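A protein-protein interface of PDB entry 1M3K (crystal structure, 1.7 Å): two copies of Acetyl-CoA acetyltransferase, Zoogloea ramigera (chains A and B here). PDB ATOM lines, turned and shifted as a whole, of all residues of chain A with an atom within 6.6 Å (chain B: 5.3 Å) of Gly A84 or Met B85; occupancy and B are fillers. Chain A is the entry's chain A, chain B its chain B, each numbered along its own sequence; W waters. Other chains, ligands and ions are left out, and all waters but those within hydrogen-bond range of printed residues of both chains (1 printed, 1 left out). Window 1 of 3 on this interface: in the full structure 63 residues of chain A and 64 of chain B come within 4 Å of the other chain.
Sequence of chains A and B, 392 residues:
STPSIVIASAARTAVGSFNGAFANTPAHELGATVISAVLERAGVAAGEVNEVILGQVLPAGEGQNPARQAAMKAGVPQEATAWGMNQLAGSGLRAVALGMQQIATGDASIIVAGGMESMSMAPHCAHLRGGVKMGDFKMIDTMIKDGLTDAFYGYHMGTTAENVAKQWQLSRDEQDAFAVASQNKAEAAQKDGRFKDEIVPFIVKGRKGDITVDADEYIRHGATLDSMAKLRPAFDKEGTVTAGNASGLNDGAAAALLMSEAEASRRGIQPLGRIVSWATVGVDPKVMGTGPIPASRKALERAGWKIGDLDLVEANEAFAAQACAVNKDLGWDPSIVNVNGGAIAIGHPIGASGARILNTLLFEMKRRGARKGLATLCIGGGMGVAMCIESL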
ATOM      1  N   VAL A  52     -31.062  -6.469   5.477  1.00  0.00           N
ATOM      2  CA  VAL A  52     -31.715  -6.301   6.753  1.00  0.00           C
ATOM      3  C   VAL A  52     -30.676  -6.056   7.852  1.00  0.00           C
ATOM      4  O   VAL A  52     -29.689  -6.723   7.971  1.00  0.00           O
ATOM      5  CB  VAL A  52     -32.518  -7.575   7.129  1.00  0.00           C
ATOM      6  CG1 VAL A  52     -33.170  -7.420   8.508  1.00  0.00           C
ATOM      7  CG2 VAL A  52     -33.575  -7.837   6.149  1.00  0.00           C
ATOM      8  N   ILE A  53     -30.901  -5.028   8.626  1.00  0.00           N
ATOM      9  CA  ILE A  53     -29.996  -4.585   9.659  1.00  0.00           C
ATOM     10  C   ILE A  53     -30.775  -4.467  10.967  1.00  0.00           C
ATOM     11  O   ILE A  53     -31.705  -3.676  11.073  1.00  0.00           O
ATOM     12  CB  ILE A  53     -29.370  -3.237   9.325  1.00  0.00           C
ATOM     13  CG1 ILE A  53     -28.781  -3.208   7.919  1.00  0.00           C
ATOM     14  CG2 ILE A  53     -28.277  -2.868  10.320  1.00  0.00           C
ATOM     15  CD1 ILE A  53     -28.373  -1.737   7.555  1.00  0.00           C
ATOM     16  N   LEU A  54     -30.403  -5.290  11.950  1.00  0.00           N
ATOM     17  CA  LEU A  54     -31.193  -5.392  13.185  1.00  0.00           C
ATOM     18  C   LEU A  54     -30.312  -5.174  14.392  1.00  0.00           C
ATOM     19  O   LEU A  54     -29.409  -5.924  14.602  1.00  0.00           O
ATOM     20  CB  LEU A  54     -31.941  -6.680  13.275  1.00  0.00           C
ATOM     21  CG  LEU A  54     -33.098  -6.911  12.249  1.00  0.00           C
ATOM     22  CD1 LEU A  54     -33.555  -8.279  12.218  1.00  0.00           C
ATOM     23  CD2 LEU A  54     -34.382  -5.959  12.496  1.00  0.00           C
ATOM     24  N   GLY A  55     -30.629  -4.190  15.206  1.00  0.00           N
ATOM     25  CA  GLY A  55     -29.922  -4.038  16.464  1.00  0.00           C
ATOM     26  C   GLY A  55     -30.335  -5.158  17.385  1.00  0.00           C
ATOM     27  O   GLY A  55     -31.478  -5.571  17.347  1.00  0.00           O
ATOM     28  N   GLN A  56     -29.386  -5.623  18.203  1.00  0.00           N
ATOM     29  CA  GLN A  56     -29.696  -6.700  19.176  1.00  0.00           C
ATOM     30  C   GLN A  56     -28.602  -6.763  20.134  1.00  0.00           C
ATOM     31  O   GLN A  56     -27.441  -6.924  19.754  1.00  0.00           O
ATOM     32  CB  GLN A  56     -29.960  -8.040  18.479  1.00  0.00           C
ATOM     33  CG  GLN A  56     -30.174  -9.214  19.452  1.00  0.00           C
ATOM     34  CD  GLN A  56     -30.490 -10.459  18.704  1.00  0.00           C
ATOM     35  OE1 GLN A  56     -30.004 -10.617  17.578  1.00  0.00           O
ATOM     36  NE2 GLN A  56     -31.221 -11.371  19.310  1.00  0.00           N
ATOM     37  N   ASN A  65     -25.889 -15.301  13.606  1.00  0.00           N
ATOM     38  CA  ASN A  65     -26.416 -14.048  13.041  1.00  0.00           C
ATOM     39  C   ASN A  65     -27.963 -14.059  13.020  1.00  0.00           C
ATOM     40  O   ASN A  65     -28.615 -14.243  11.964  1.00  0.00           O
ATOM     41  CB  ASN A  65     -25.821 -13.876  11.616  1.00  0.00           C
ATOM     42  CG  ASN A  65     -26.151 -12.503  10.956  1.00  0.00           C
ATOM     43  OD1 ASN A  65     -26.679 -11.576  11.585  1.00  0.00           O
ATOM     44  ND2 ASN A  65     -25.906 -12.426   9.634  1.00  0.00           N
ATOM     45  N   ALA A  67     -30.033 -11.827  12.800  1.00  0.00           N
ATOM     46  CA  ALA A  67     -30.635 -10.944  11.757  1.00  0.00           C
ATOM     47  C   ALA A  67     -30.895 -11.717  10.463  1.00  0.00           C
ATOM     48  O   ALA A  67     -31.893 -11.506   9.762  1.00  0.00           O
ATOM     49  CB  ALA A  67     -29.719  -9.797  11.419  1.00  0.00           C
ATOM     50  N   ARG A  68     -29.900 -12.505  10.078  1.00  0.00           N
ATOM     51  CA  ARG A  68     -30.111 -13.345   8.869  1.00  0.00           C
ATOM     52  C   ARG A  68     -31.219 -14.368   9.050  1.00  0.00           C
ATOM     53  O   ARG A  68     -31.967 -14.710   8.115  1.00  0.00           O
ATOM     54  CB  ARG A  68     -28.797 -14.078   8.580  1.00  0.00           C
ATOM     55  CG  ARG A  68     -28.806 -15.012   7.374  1.00  0.00           C
ATOM     56  CD  ARG A  68     -28.899 -14.316   6.006  1.00  0.00           C
ATOM     57  NE  ARG A  68     -28.446 -15.232   4.967  1.00  0.00           N
ATOM     58  CZ  ARG A  68     -28.533 -14.920   3.650  1.00  0.00           C
ATOM     59  NH1 ARG A  68     -28.992 -13.750   3.271  1.00  0.00           N
ATOM     60  NH2 ARG A  68     -27.996 -15.705   2.774  1.00  0.00           N
ATOM     61  N   ALA A  82     -27.654  -9.584   5.600  1.00  0.00           N
ATOM     62  CA  ALA A  82     -28.302  -9.277   6.882  1.00  0.00           C
ATOM     63  C   ALA A  82     -27.209  -9.234   7.889  1.00  0.00           C
ATOM     64  O   ALA A  82     -26.289 -10.035   7.822  1.00  0.00           O
ATOM     65  CB  ALA A  82     -29.262 -10.302   7.230  1.00  0.00           C
ATOM     66  N   TRP A  83     -27.295  -8.300   8.843  1.00  0.00           N
ATOM     67  CA  TRP A  83     -26.332  -8.297   9.921  1.00  0.00           C
ATOM     68  C   TRP A  83     -26.923  -7.668  11.141  1.00  0.00           C
ATOM     69  O   TRP A  83     -27.930  -6.966  11.044  1.00  0.00           O
ATOM     70  CB  TRP A  83     -25.047  -7.549   9.509  1.00  0.00           C
ATOM     71  CG  TRP A  83     -25.199  -6.192   8.833  1.00  0.00           C
ATOM     72  CD1 TRP A  83     -25.600  -5.958   7.539  1.00  0.00           C
ATOM     73  CD2 TRP A  83     -24.982  -4.899   9.419  1.00  0.00           C
ATOM     74  NE1 TRP A  83     -25.584  -4.617   7.267  1.00  0.00           N
ATOM     75  CE2 TRP A  83     -25.164  -3.953   8.400  1.00  0.00           C
ATOM     76  CE3 TRP A  83     -24.555  -4.451  10.704  1.00  0.00           C
ATOM     77  CZ2 TRP A  83     -25.028  -2.594   8.610  1.00  0.00           C
ATOM     78  CZ3 TRP A  83     -24.433  -3.106  10.912  1.00  0.00           C
ATOM     79  CH2 TRP A  83     -24.626  -2.196   9.867  1.00  0.00           C
ATOM     80  N   GLY A  84     -26.306  -7.928  12.270  1.00  0.00           N
ATOM     81  CA  GLY A  84     -26.717  -7.358  13.553  1.00  0.00           C
ATOM     82  C   GLY A  84     -25.736  -6.363  14.098  1.00  0.00           C
ATOM     83  O   GLY A  84     -24.567  -6.313  13.702  1.00  0.00           O
ATOM     84  N   MET A  85     -26.219  -5.461  14.941  1.00  0.00           N
ATOM     85  CA  MET A  85     -25.333  -4.491  15.551  1.00  0.00           C
ATOM     86  C   MET A  85     -25.744  -4.116  16.934  1.00  0.00           C
ATOM     87  O   MET A  85     -26.883  -4.395  17.325  1.00  0.00           O
ATOM     88  CB  MET A  85     -25.048  -3.241  14.705  1.00  0.00           C
ATOM     89  CG  MET A  85     -26.308  -2.518  14.145  1.00  0.00           C
ATOM     90  SD  MET A  85     -27.112  -1.493  15.422  1.00  0.00           S
ATOM     91  CE  MET A  85     -25.888  -0.421  15.890  1.00  0.00           C
ATOM     92  N   ASN A  86     -24.787  -3.568  17.708  1.00  0.00           N
ATOM     93  CA  ASN A  86     -25.021  -3.246  19.110  1.00  0.00           C
ATOM     94  C   ASN A  86     -24.367  -1.943  19.568  1.00  0.00           C
ATOM     95  O   ASN A  86     -23.140  -1.834  19.736  1.00  0.00           O
ATOM     96  CB  ASN A  86     -24.581  -4.445  19.958  1.00  0.00           C
ATOM     97  CG  ASN A  86     -24.620  -4.183  21.458  1.00  0.00           C
ATOM     98  OD1 ASN A  86     -25.377  -3.346  21.884  1.00  0.00           O
ATOM     99  ND2 ASN A  86     -23.889  -5.016  22.272  1.00  0.00           N
ATOM    100  N   ILE B  53     -15.697   1.296  15.562  1.00  0.00           N
ATOM    101  CA  ILE B  53     -16.648   0.312  15.080  1.00  0.00           C
ATOM    102  C   ILE B  53     -15.936  -1.029  14.982  1.00  0.00           C
ATOM    103  O   ILE B  53     -14.893  -1.147  14.273  1.00  0.00           O
ATOM    104  CB  ILE B  53     -17.154   0.688  13.700  1.00  0.00           C
ATOM    105  CG1 ILE B  53     -17.759   2.097  13.592  1.00  0.00           C
ATOM    106  CG2 ILE B  53     -18.156  -0.394  13.249  1.00  0.00           C
ATOM    107  CD1 ILE B  53     -18.100   2.410  12.091  1.00  0.00           C
ATOM    108  N   LEU B  54     -16.378  -2.023  15.781  1.00  0.00           N
ATOM    109  CA  LEU B  54     -15.582  -3.278  15.913  1.00  0.00           C
ATOM    110  C   LEU B  54     -16.518  -4.464  15.705  1.00  0.00           C
ATOM    111  O   LEU B  54     -17.425  -4.702  16.499  1.00  0.00           O
ATOM    112  CB  LEU B  54     -14.862  -3.441  17.241  1.00  0.00           C
ATOM    113  CG  LEU B  54     -13.710  -2.437  17.490  1.00  0.00           C
ATOM    114  CD1 LEU B  54     -13.297  -2.298  18.855  1.00  0.00           C
ATOM    115  CD2 LEU B  54     -12.556  -2.755  16.506  1.00  0.00           C
ATOM    116  N   GLY B  55     -16.248  -5.263  14.667  1.00  0.00           N
ATOM    117  CA  GLY B  55     -16.957  -6.516  14.510  1.00  0.00           C
ATOM    118  C   GLY B  55     -16.542  -7.472  15.623  1.00  0.00           C
ATOM    119  O   GLY B  55     -15.381  -7.496  16.154  1.00  0.00           O
ATOM    120  N   GLN B  56     -17.510  -8.297  16.022  1.00  0.00           N
ATOM    121  CA  GLN B  56     -17.297  -9.246  17.144  1.00  0.00           C
ATOM    122  C   GLN B  56     -18.488 -10.142  17.138  1.00  0.00           C
ATOM    123  O   GLN B  56     -19.661  -9.659  17.220  1.00  0.00           O
ATOM    124  CB  GLN B  56     -17.152  -8.571  18.497  1.00  0.00           C
ATOM    125  CG  GLN B  56     -16.877  -9.496  19.611  1.00  0.00           C
ATOM    126  CD  GLN B  56     -16.715  -8.799  20.934  1.00  0.00           C
ATOM    127  OE1 GLN B  56     -17.223  -7.679  21.120  1.00  0.00           O
ATOM    128  NE2 GLN B  56     -16.073  -9.471  21.895  1.00  0.00           N
ATOM    129  N   VAL B  57     -18.209 -11.435  17.024  1.00  0.00           N
ATOM    130  CA  VAL B  57     -19.258 -12.469  16.903  1.00  0.00           C
ATOM    131  C   VAL B  57     -19.653 -13.055  18.239  1.00  0.00           C
ATOM    132  O   VAL B  57     -20.818 -13.373  18.457  1.00  0.00           O
ATOM    133  CB  VAL B  57     -18.854 -13.516  15.905  1.00  0.00           C
ATOM    134  CG1 VAL B  57     -20.000 -14.627  15.708  1.00  0.00           C
ATOM    135  CG2 VAL B  57     -18.497 -12.843  14.631  1.00  0.00           C
ATOM    136  N   TRP B  83     -19.445   1.168  18.761  1.00  0.00           N
ATOM    137  CA  TRP B  83     -20.460   0.132  18.610  1.00  0.00           C
ATOM    138  C   TRP B  83     -19.863  -1.127  18.014  1.00  0.00           C
ATOM    139  O   TRP B  83     -18.782  -1.055  17.458  1.00  0.00           O
ATOM    140  CB  TRP B  83     -21.646   0.662  17.823  1.00  0.00           C
ATOM    141  CG  TRP B  83     -21.406   1.325  16.524  1.00  0.00           C
ATOM    142  CD1 TRP B  83     -20.953   2.594  16.329  1.00  0.00           C
ATOM    143  CD2 TRP B  83     -21.658   0.767  15.224  1.00  0.00           C
ATOM    144  NE1 TRP B  83     -20.887   2.853  14.980  1.00  0.00           N
ATOM    145  CE2 TRP B  83     -21.352   1.761  14.280  1.00  0.00           C
ATOM    146  CE3 TRP B  83     -22.121  -0.466  14.762  1.00  0.00           C
ATOM    147  CZ2 TRP B  83     -21.446   1.537  12.905  1.00  0.00           C
ATOM    148  CZ3 TRP B  83     -22.268  -0.676  13.375  1.00  0.00           C
ATOM    149  CH2 TRP B  83     -21.907   0.316  12.487  1.00  0.00           C
ATOM    150  N   GLY B  84     -20.466  -2.284  18.266  1.00  0.00           N
ATOM    151  CA  GLY B  84     -20.106  -3.510  17.629  1.00  0.00           C
ATOM    152  C   GLY B  84     -21.115  -3.964  16.652  1.00  0.00           C
ATOM    153  O   GLY B  84     -22.324  -3.498  16.489  1.00  0.00           O
ATOM    154  N   MET B  85     -20.595  -4.869  15.844  1.00  0.00           N
ATOM    155  CA  MET B  85     -21.450  -5.405  14.813  1.00  0.00           C
ATOM    156  C   MET B  85     -21.076  -6.856  14.467  1.00  0.00           C
ATOM    157  O   MET B  85     -20.001  -7.314  14.774  1.00  0.00           O
ATOM    158  CB  MET B  85     -21.559  -4.521  13.566  1.00  0.00           C
ATOM    159  CG  MET B  85     -20.252  -4.047  12.809  1.00  0.00           C
ATOM    160  SD  MET B  85     -19.530  -5.397  11.809  1.00  0.00           S
ATOM    161  CE  MET B  85     -20.851  -5.697  10.752  1.00  0.00           C
ATOM    162  N   ASN B  86     -22.014  -7.530  13.824  1.00  0.00           N
ATOM    163  CA  ASN B  86     -21.846  -8.948  13.474  1.00  0.00           C
ATOM    164  C   ASN B  86     -22.422  -9.336  12.154  1.00  0.00           C
ATOM    165  O   ASN B  86     -23.650  -9.340  11.977  1.00  0.00           O
ATOM    166  CB  ASN B  86     -22.512  -9.769  14.621  1.00  0.00           C
ATOM    167  CG  ASN B  86     -22.476 -11.256  14.370  1.00  0.00           C
ATOM    168  OD1 ASN B  86     -21.750 -11.723  13.503  1.00  0.00           O
ATOM    169  ND2 ASN B  86     -23.215 -12.028  15.164  1.00  0.00           N
ATOM    170  N   GLN B  87     -21.538  -9.496  11.152  1.00  0.00           N
ATOM    171  CA  GLN B  87     -21.842 -10.145   9.904  1.00  0.00           C
ATOM    172  C   GLN B  87     -20.830 -11.373   9.908  1.00  0.00           C
ATOM    173  O   GLN B  87     -20.219 -11.580   8.909  1.00  0.00           O
ATOM    174  CB  GLN B  87     -21.686  -9.230   8.660  1.00  0.00           C
ATOM    175  CG  GLN B  87     -22.380  -9.722   7.368  1.00  0.00           C
ATOM    176  CD  GLN B  87     -22.282  -8.796   6.171  1.00  0.00           C
ATOM    177  OE1 GLN B  87     -21.687  -7.715   6.245  1.00  0.00           O
ATOM    178  NE2 GLN B  87     -22.875  -9.235   5.029  1.00  0.00           N
ATOM    179  N   SER B  91     -17.367  -9.723   9.452  1.00  0.00           N
ATOM    180  CA  SER B  91     -17.490  -8.555  10.323  1.00  0.00           C
ATOM    181  C   SER B  91     -16.310  -7.563  10.306  1.00  0.00           C
ATOM    182  O   SER B  91     -16.523  -6.385  10.275  1.00  0.00           O
ATOM    183  CB  SER B  91     -17.648  -8.975  11.758  1.00  0.00           C
ATOM    184  OG  SER B  91     -18.760  -9.836  11.923  1.00  0.00           O
ATOM    185  N   ARG B  94     -16.386  -5.699   7.062  1.00  0.00           N
ATOM    186  CA  ARG B  94     -17.611  -4.915   6.874  1.00  0.00           C
ATOM    187  C   ARG B  94     -17.531  -3.657   7.758  1.00  0.00           C
ATOM    188  O   ARG B  94     -17.981  -2.583   7.355  1.00  0.00           O
ATOM    189  CB  ARG B  94     -18.848  -5.762   7.222  1.00  0.00           C
ATOM    190  CG  ARG B  94     -20.152  -4.996   7.118  1.00  0.00           C
ATOM    191  CD  ARG B  94     -20.382  -4.611   5.690  1.00  0.00           C
ATOM    192  NE  ARG B  94     -21.487  -3.697   5.445  1.00  0.00           N
ATOM    193  CZ  ARG B  94     -22.748  -4.040   5.199  1.00  0.00           C
ATOM    194  NH1 ARG B  94     -23.132  -5.268   5.273  1.00  0.00           N
ATOM    195  NH2 ARG B  94     -23.634  -3.128   4.920  1.00  0.00           N
ATOM    196  N   ALA B  95     -16.893  -3.757   8.915  1.00  0.00           N
ATOM    197  CA  ALA B  95     -16.766  -2.626   9.826  1.00  0.00           C
ATOM    198  C   ALA B  95     -15.999  -1.524   9.177  1.00  0.00           C
ATOM    199  O   ALA B  95     -16.313  -0.349   9.376  1.00  0.00           O
ATOM    200  CB  ALA B  95     -16.098  -3.070  11.131  1.00  0.00           C
ATOM    201  N   LEU B  98     -18.266   0.188   6.753  1.00  0.00           N
ATOM    202  CA  LEU B  98     -19.216   0.973   7.545  1.00  0.00           C
ATOM    203  C   LEU B  98     -18.615   2.272   8.063  1.00  0.00           C
ATOM    204  O   LEU B  98     -19.236   3.297   8.129  1.00  0.00           O
ATOM    205  CB  LEU B  98     -19.732   0.090   8.695  1.00  0.00           C
ATOM    206  CG  LEU B  98     -20.721  -1.006   8.379  1.00  0.00           C
ATOM    207  CD1 LEU B  98     -20.947  -1.949   9.569  1.00  0.00           C
ATOM    208  CD2 LEU B  98     -22.025  -0.387   8.015  1.00  0.00           C
HETATM  209  O   HOH W   1     -23.708 -14.989  15.434  1.00  0.00           O
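N of Leu A54 sits at hydrogen-bond distance from O of Trp A83 (3.1 Å). N of Met A85 is in hydrogen-bond range of O of Leu A54 (3.2 Å). The side-chain amide nitrogen (ND2) of Asn A65 is in hydrogen-bond range of the backbone carbonyl oxygen (O) of Ala A82, 3.0 Å away. O of Met B85 is in hydrogen-bond range of N of Gln B56, at 3.0 Å. N of Gln B87 is in hydrogen-bond range of OG of Ser B91 (2.9 Å). The guanidinium group (NH1) of Arg B94 is in hydrogen-bond range of the side-chain amide oxygen (OE1) of Gln B87.
Of the 13 printed residues of chain A, 6 touch a printed residue of chain B. Printed residues of chain A that touch a printed residue of chain B: Asn A65, Ala A82, Trp A83, Gly A84, Met A85 and Asn A86. Along chain A the printed residues that touch a printed residue of chain B span positions 65 to 86. Printed residues of chain B that touch a printed residue of chain A: Trp B83, Gly B84, Met B85, Asn B86, Gln B87, Arg B94 and Leu B98. Hydrophobic or aromatic side chains of chain B that line the printed part of chain A: Trp B83, Met B85 and Leu B98. Among the printed residues, 14 pairs touch across the chains. Among the printed residues, no Asp or Glu carboxylate lies within 4 Å of a Lys or Arg side-chain nitrogen of the other chain.
Gly A84 touches just these residues of chain B: Met B85 and Asn B86. Met B85 touches three residues of chain A. Of the printed residues of chain B, Ala A82 touches Gln B87 (3.9 Å). Of the printed residues of chain A, Arg B94 touches Trp A83. Of the printed residues of chain A, Trp B83 touches Met A85 and Asn A86. The nearest printed residue of chain B that does not touch Asn A86 is Met B85 (4.8 Å).
Asn A65 touches Asn B86 (OD1 to O, 3.8 Å). CG of Gln B87 touches O of Ala A82 (3.9 Å). CE of Met B85 touches CE3 of Trp A83, at 3.9 Å. Trp A83 touches Asn B86. Gln B87 touches Trp A83 (CB to CB, 3.9 Å). CH2 of Trp A83 touches CD2 of Leu B98 (3.7 Å). Met B85 touches Gly A84. CE of Met A85 touches CE3 of Trp B83, 3.9 Å away. CB of Met A85 touches O of Gly B84, at 3.3 Å. CB of Met B85 touches CB of Met A85, 3.9 Å away.
Water W1 bridges the backbone NH (N) of Asn A65 (2.9 Å) and the side-chain amide nitrogen (ND2) of Asn B86 (3.0 Å).
Trp A83 touches Met B85, and with the chains exchanged Met A85 touches Trp B83. Trp A83 touches Asn B86, and with the chains exchanged Asn A86 touches Trp B83. Gly A84 touches Asn B86, and with the chains exchanged Asn A86 touches Gly B84. Met B85 touches its own counterpart, Met A85.
The backbone NH of Asn B86 lies within hydrogen-bond range of the backbone carbonyl oxygen of Gly A84 (2.8 Å). The backbone NH (N) of Asn A86 is in hydrogen-bond range of the backbone carbonyl oxygen (O) of Gly B84 (2.7 Å). The indole nitrogen of Trp A83 sits close to the guanidinium group of Arg B94 (3.2 Å).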
